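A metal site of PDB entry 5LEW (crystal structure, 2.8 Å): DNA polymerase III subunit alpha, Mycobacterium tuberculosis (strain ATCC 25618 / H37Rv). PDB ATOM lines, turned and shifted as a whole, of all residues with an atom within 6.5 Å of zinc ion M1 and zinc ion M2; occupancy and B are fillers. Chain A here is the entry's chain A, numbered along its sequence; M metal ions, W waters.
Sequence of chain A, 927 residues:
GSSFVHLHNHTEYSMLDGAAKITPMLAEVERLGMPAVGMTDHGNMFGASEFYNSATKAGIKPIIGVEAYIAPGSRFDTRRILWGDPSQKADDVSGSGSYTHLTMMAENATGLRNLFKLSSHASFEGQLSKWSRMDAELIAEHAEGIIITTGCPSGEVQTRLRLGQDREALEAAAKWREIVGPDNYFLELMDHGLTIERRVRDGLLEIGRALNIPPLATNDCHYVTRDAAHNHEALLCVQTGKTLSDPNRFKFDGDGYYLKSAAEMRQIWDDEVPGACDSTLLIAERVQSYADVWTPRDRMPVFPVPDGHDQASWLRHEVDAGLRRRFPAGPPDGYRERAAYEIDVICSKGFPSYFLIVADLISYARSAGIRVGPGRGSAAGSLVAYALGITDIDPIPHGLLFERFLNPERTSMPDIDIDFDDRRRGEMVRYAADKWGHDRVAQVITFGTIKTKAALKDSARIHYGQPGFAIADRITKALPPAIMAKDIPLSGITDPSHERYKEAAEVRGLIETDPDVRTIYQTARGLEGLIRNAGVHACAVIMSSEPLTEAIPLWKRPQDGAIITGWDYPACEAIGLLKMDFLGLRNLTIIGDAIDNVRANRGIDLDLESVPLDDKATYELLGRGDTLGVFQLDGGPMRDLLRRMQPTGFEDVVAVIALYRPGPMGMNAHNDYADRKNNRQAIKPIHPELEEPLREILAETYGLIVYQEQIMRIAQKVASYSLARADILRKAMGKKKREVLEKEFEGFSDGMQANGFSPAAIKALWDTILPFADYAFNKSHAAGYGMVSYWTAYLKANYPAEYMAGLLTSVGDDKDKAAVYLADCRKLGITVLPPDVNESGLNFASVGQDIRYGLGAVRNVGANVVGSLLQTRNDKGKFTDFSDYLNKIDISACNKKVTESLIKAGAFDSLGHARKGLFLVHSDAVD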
ATOM      1  N   HIS A   8       1.289 -32.633 -24.112  1.00  0.00           N
ATOM      2  CA  HIS A   8       0.753 -31.326 -24.475  1.00  0.00           C
ATOM      3  C   HIS A   8       1.862 -30.288 -24.592  1.00  0.00           C
ATOM      4  O   HIS A   8       2.479 -29.887 -23.620  1.00  0.00           O
ATOM      5  CB  HIS A   8      -0.253 -30.917 -23.425  1.00  0.00           C
ATOM      6  CG  HIS A   8      -1.034 -29.699 -23.779  1.00  0.00           C
ATOM      7  ND1 HIS A   8      -2.367 -29.567 -23.447  1.00  0.00           N
ATOM      8  CD2 HIS A   8      -0.690 -28.577 -24.457  1.00  0.00           C
ATOM      9  CE1 HIS A   8      -2.807 -28.396 -23.880  1.00  0.00           C
ATOM     10  NE2 HIS A   8      -1.816 -27.804 -24.525  1.00  0.00           N
ATOM     11  N   ASN A   9       2.088 -29.822 -25.811  1.00  0.00           N
ATOM     12  CA  ASN A   9       3.301 -29.043 -26.147  1.00  0.00           C
ATOM     13  C   ASN A   9       3.187 -28.086 -27.304  1.00  0.00           C
ATOM     14  O   ASN A   9       2.723 -28.476 -28.366  1.00  0.00           O
ATOM     15  CB  ASN A   9       4.312 -29.994 -26.676  1.00  0.00           C
ATOM     16  CG  ASN A   9       5.246 -30.361 -25.680  1.00  0.00           C
ATOM     17  OD1 ASN A   9       5.903 -29.498 -25.170  1.00  0.00           O
ATOM     18  ND2 ASN A   9       5.344 -31.638 -25.367  1.00  0.00           N
ATOM     19  N   HIS A  10       3.708 -26.865 -27.140  1.00  0.00           N
ATOM     20  CA  HIS A  10       3.595 -25.841 -28.190  1.00  0.00           C
ATOM     21  C   HIS A  10       4.907 -25.435 -28.809  1.00  0.00           C
ATOM     22  O   HIS A  10       5.778 -24.896 -28.161  1.00  0.00           O
ATOM     23  CB  HIS A  10       2.836 -24.643 -27.708  1.00  0.00           C
ATOM     24  CG  HIS A  10       1.432 -24.946 -27.311  1.00  0.00           C
ATOM     25  ND1 HIS A  10       0.378 -24.743 -28.151  1.00  0.00           N
ATOM     26  CD2 HIS A  10       0.914 -25.460 -26.155  1.00  0.00           C
ATOM     27  CE1 HIS A  10      -0.751 -25.068 -27.524  1.00  0.00           C
ATOM     28  NE2 HIS A  10      -0.447 -25.528 -26.324  1.00  0.00           N
ATOM     29  N   THR A  40       1.456 -30.328 -30.026  1.00  0.00           N
ATOM     30  CA  THR A  40       0.056 -29.955 -29.814  1.00  0.00           C
ATOM     31  C   THR A  40      -0.143 -28.498 -30.158  1.00  0.00           C
ATOM     32  O   THR A  40      -0.326 -27.664 -29.280  1.00  0.00           O
ATOM     33  CB  THR A  40      -0.289 -30.253 -28.335  1.00  0.00           C
ATOM     34  OG1 THR A  40      -0.550 -31.616 -28.280  1.00  0.00           O
ATOM     35  CG2 THR A  40      -1.562 -29.626 -27.930  1.00  0.00           C
ATOM     36  N   HIS A  42      -1.564 -24.780 -31.489  1.00  0.00           N
ATOM     37  CA  HIS A  42      -2.871 -24.163 -31.412  1.00  0.00           C
ATOM     38  C   HIS A  42      -3.469 -24.090 -32.784  1.00  0.00           C
ATOM     39  O   HIS A  42      -3.086 -23.290 -33.604  1.00  0.00           O
ATOM     40  CB  HIS A  42      -2.780 -22.743 -30.882  1.00  0.00           C
ATOM     41  CG  HIS A  42      -2.558 -22.653 -29.413  1.00  0.00           C
ATOM     42  ND1 HIS A  42      -3.487 -23.092 -28.510  1.00  0.00           N
ATOM     43  CD2 HIS A  42      -1.540 -22.145 -28.696  1.00  0.00           C
ATOM     44  CE1 HIS A  42      -3.043 -22.870 -27.290  1.00  0.00           C
ATOM     45  NE2 HIS A  42      -1.855 -22.298 -27.376  1.00  0.00           N
ATOM     46  N   GLU A  67      -3.718 -28.946 -30.548  1.00  0.00           N
ATOM     47  CA  GLU A  67      -4.693 -28.353 -29.667  1.00  0.00           C
ATOM     48  C   GLU A  67      -5.744 -27.605 -30.457  1.00  0.00           C
ATOM     49  O   GLU A  67      -5.596 -26.403 -30.732  1.00  0.00           O
ATOM     50  CB  GLU A  67      -4.055 -27.463 -28.629  1.00  0.00           C
ATOM     51  CG  GLU A  67      -5.002 -27.229 -27.454  1.00  0.00           C
ATOM     52  CD  GLU A  67      -4.355 -26.524 -26.289  1.00  0.00           C
ATOM     53  OE1 GLU A  67      -3.164 -26.114 -26.373  1.00  0.00           O
ATOM     54  OE2 GLU A  67      -5.111 -26.379 -25.293  1.00  0.00           O
ATOM     55  N   HIS A 101     -10.246 -24.823 -25.945  1.00  0.00           N
ATOM     56  CA  HIS A 101      -9.186 -25.756 -26.346  1.00  0.00           C
ATOM     57  C   HIS A 101      -9.543 -27.215 -26.235  1.00  0.00           C
ATOM     58  O   HIS A 101     -10.417 -27.576 -25.433  1.00  0.00           O
ATOM     59  CB  HIS A 101      -7.996 -25.573 -25.446  1.00  0.00           C
ATOM     60  CG  HIS A 101      -7.375 -24.237 -25.557  1.00  0.00           C
ATOM     61  ND1 HIS A 101      -6.205 -23.943 -24.917  1.00  0.00           N
ATOM     62  CD2 HIS A 101      -7.772 -23.107 -26.206  1.00  0.00           C
ATOM     63  CE1 HIS A 101      -5.874 -22.687 -25.176  1.00  0.00           C
ATOM     64  NE2 HIS A 101      -6.815 -22.155 -25.954  1.00  0.00           N
ATOM     65  N   LEU A 102      -8.882 -28.068 -27.022  1.00  0.00           N
ATOM     66  CA  LEU A 102      -9.007 -29.493 -26.903  1.00  0.00           C
ATOM     67  C   LEU A 102      -7.714 -30.138 -27.340  1.00  0.00           C
ATOM     68  O   LEU A 102      -7.279 -29.905 -28.462  1.00  0.00           O
ATOM     69  CB  LEU A 102     -10.149 -29.961 -27.788  1.00  0.00           C
ATOM     70  CG  LEU A 102     -10.418 -31.476 -27.704  1.00  0.00           C
ATOM     71  CD1 LEU A 102     -10.697 -31.892 -26.264  1.00  0.00           C
ATOM     72  CD2 LEU A 102     -11.479 -31.961 -28.685  1.00  0.00           C
ATOM     73  N   THR A 103      -7.127 -30.937 -26.475  1.00  0.00           N
ATOM     74  CA  THR A 103      -5.827 -31.580 -26.750  1.00  0.00           C
ATOM     75  C   THR A 103      -6.137 -32.865 -27.489  1.00  0.00           C
ATOM     76  O   THR A 103      -6.866 -33.692 -26.929  1.00  0.00           O
ATOM     77  CB  THR A 103      -5.192 -31.962 -25.422  1.00  0.00           C
ATOM     78  OG1 THR A 103      -5.383 -30.865 -24.523  1.00  0.00           O
ATOM     79  CG2 THR A 103      -3.713 -32.316 -25.528  1.00  0.00           C
ATOM     80  N   GLY A 151      -8.907 -31.565 -21.341  1.00  0.00           N
ATOM     81  CA  GLY A 151      -8.343 -30.291 -21.706  1.00  0.00           C
ATOM     82  C   GLY A 151      -7.690 -29.480 -20.630  1.00  0.00           C
ATOM     83  O   GLY A 151      -7.820 -29.814 -19.448  1.00  0.00           O
ATOM     84  N   CYS A 152      -6.954 -28.451 -21.079  1.00  0.00           N
ATOM     85  CA  CYS A 152      -6.334 -27.383 -20.319  1.00  0.00           C
ATOM     86  C   CYS A 152      -7.421 -26.510 -19.666  1.00  0.00           C
ATOM     87  O   CYS A 152      -8.608 -26.737 -19.869  1.00  0.00           O
ATOM     88  CB  CYS A 152      -5.445 -26.527 -21.268  1.00  0.00           C
ATOM     89  SG  CYS A 152      -6.258 -25.259 -22.306  1.00  0.00           S
ATOM     90  N   PRO A 153      -7.032 -25.485 -18.896  1.00  0.00           N
ATOM     91  CA  PRO A 153      -8.078 -24.627 -18.363  1.00  0.00           C
ATOM     92  C   PRO A 153      -8.928 -23.970 -19.411  1.00  0.00           C
ATOM     93  O   PRO A 153     -10.086 -23.796 -19.185  1.00  0.00           O
ATOM     94  CB  PRO A 153      -7.326 -23.550 -17.605  1.00  0.00           C
ATOM     95  CG  PRO A 153      -6.064 -24.258 -17.208  1.00  0.00           C
ATOM     96  CD  PRO A 153      -5.721 -25.200 -18.311  1.00  0.00           C
ATOM     97  N   SER A 154      -8.416 -23.613 -20.575  1.00  0.00           N
ATOM     98  CA  SER A 154      -9.301 -23.038 -21.578  1.00  0.00           C
ATOM     99  C   SER A 154     -10.152 -24.086 -22.279  1.00  0.00           C
ATOM    100  O   SER A 154     -10.868 -23.743 -23.244  1.00  0.00           O
ATOM    101  CB  SER A 154      -8.495 -22.300 -22.619  1.00  0.00           C
ATOM    102  OG  SER A 154      -8.051 -21.071 -22.157  1.00  0.00           O
ATOM    103  N   GLY A 155     -10.046 -25.346 -21.853  1.00  0.00           N
ATOM    104  CA  GLY A 155     -10.983 -26.385 -22.278  1.00  0.00           C
ATOM    105  C   GLY A 155     -12.439 -26.211 -21.768  1.00  0.00           C
ATOM    106  O   GLY A 155     -12.693 -25.412 -20.866  1.00  0.00           O
ATOM    107  N   MET A 190      -2.795 -30.555 -14.867  1.00  0.00           N
ATOM    108  CA  MET A 190      -1.795 -29.593 -15.191  1.00  0.00           C
ATOM    109  C   MET A 190      -1.558 -28.813 -13.911  1.00  0.00           C
ATOM    110  O   MET A 190      -2.518 -28.244 -13.295  1.00  0.00           O
ATOM    111  CB  MET A 190      -2.496 -28.716 -16.190  1.00  0.00           C
ATOM    112  CG  MET A 190      -1.685 -27.692 -16.923  1.00  0.00           C
ATOM    113  SD  MET A 190      -2.570 -27.149 -18.403  1.00  0.00           S
ATOM    114  CE  MET A 190      -2.544 -28.664 -19.426  1.00  0.00           C
ATOM    115  N   ASP A 220       1.701 -28.461 -20.894  1.00  0.00           N
ATOM    116  CA  ASP A 220       1.309 -27.335 -21.763  1.00  0.00           C
ATOM    117  C   ASP A 220       2.565 -26.435 -22.030  1.00  0.00           C
ATOM    118  O   ASP A 220       2.545 -25.210 -21.865  1.00  0.00           O
ATOM    119  CB  ASP A 220       0.219 -26.473 -21.048  1.00  0.00           C
ATOM    120  CG  ASP A 220      -0.731 -25.798 -22.021  1.00  0.00           C
ATOM    121  OD1 ASP A 220      -0.564 -26.010 -23.254  1.00  0.00           O
ATOM    122  OD2 ASP A 220      -1.683 -25.128 -21.567  1.00  0.00           O
ATOM    123  N   CYS A 221       3.665 -27.077 -22.359  1.00  0.00           N
ATOM    124  CA  CYS A 221       4.911 -26.374 -22.541  1.00  0.00           C
ATOM    125  C   CYS A 221       4.788 -25.395 -23.674  1.00  0.00           C
ATOM    126  O   CYS A 221       4.364 -25.777 -24.753  1.00  0.00           O
ATOM    127  CB  CYS A 221       6.037 -27.357 -22.853  1.00  0.00           C
ATOM    128  SG  CYS A 221       6.030 -28.825 -21.780  1.00  0.00           S
ATOM    129  N   HIS A 222       5.118 -24.135 -23.406  1.00  0.00           N
ATOM    130  CA  HIS A 222       5.214 -23.112 -24.424  1.00  0.00           C
ATOM    131  C   HIS A 222       6.690 -22.702 -24.690  1.00  0.00           C
ATOM    132  O   HIS A 222       6.945 -21.855 -25.525  1.00  0.00           O
ATOM    133  CB  HIS A 222       4.327 -21.917 -24.053  1.00  0.00           C
ATOM    134  CG  HIS A 222       2.865 -22.086 -24.386  1.00  0.00           C
ATOM    135  ND1 HIS A 222       1.996 -22.802 -23.586  1.00  0.00           N
ATOM    136  CD2 HIS A 222       2.117 -21.605 -25.412  1.00  0.00           C
ATOM    137  CE1 HIS A 222       0.787 -22.789 -24.138  1.00  0.00           C
ATOM    138  NE2 HIS A 222       0.832 -22.082 -25.243  1.00  0.00           N
HETATM  139 ZN    ZN M   1      -1.873 -25.800 -24.811  1.00  0.00          ZN
HETATM  140 ZN    ZN M   2      -4.658 -24.986 -24.017  1.00  0.00          ZN
HETATM  141 ZN    ZN M   3      -0.831 -21.267 -25.874  1.00  0.00          ZN
HETATM  142  O   HOH W   1      -2.337 -23.550 -24.280  1.00  0.00           O
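Of the 18 residues printed, 4 come within 4 Å of zinc ion M1.
Zinc ion M2 is bound by OE2 of Glu 67 (1.9 Å). Zinc ion M2 is bound by ND1 of His 101 (2.1 Å). Zinc ion M2 is bound by SG of Cys 152, 2.4 Å away. Slightly farther from zinc ion M2 lies water W1 (2.7 Å).
Zinc ion M1 is bound by a ring nitrogen (NE2) of His 8 (2.0 Å). OD1 of Asp 220 is bound to zinc ion M1. OE1 of Glu 67 binds zinc ion M1 (2.1 Å). Zinc ion M1 is bound by a ring nitrogen (NE2) of His 10 (2.1 Å). Zinc ion M1 is bound by water W1 (2.4 Å). Zinc ion M1 has five donor atoms within binding distance.
Five residues have an atom within 4 Å of zinc ion M2: His 8, Glu 67, His 101, Cys 152 and Asp 220. The nearest printed residue that does not touch zinc ion M2 is His 42 (4.2 Å).
ND1 of His 8 lies within hydrogen-bond range of OG1 of Thr 103 (3.5 Å). The backbone carbonyl oxygen (O) of His 8 sits at hydrogen-bond distance from the backbone NH (N) of Cys 221, 3.3 Å away. O of Asp 220 lies within hydrogen-bond range of ND1 of His 222. N of His 101 lies within hydrogen-bond range of O of Ser 154 (3.0 Å). A ring nitrogen (NE2) of His 42 sits close to a ring nitrogen (ND1) of His 10 (3.4 Å). A ring nitrogen (ND1) of His 10 sits close to the backbone carbonyl oxygen (O) of Thr 40. The backbone NH (N) of His 10 is in hydrogen-bond range of the backbone carbonyl oxygen (O) of Cys 221 (2.7 Å). The side-chain sulfur of Cys 152 lies close to the backbone NH of Ser 154 (3.2 Å).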
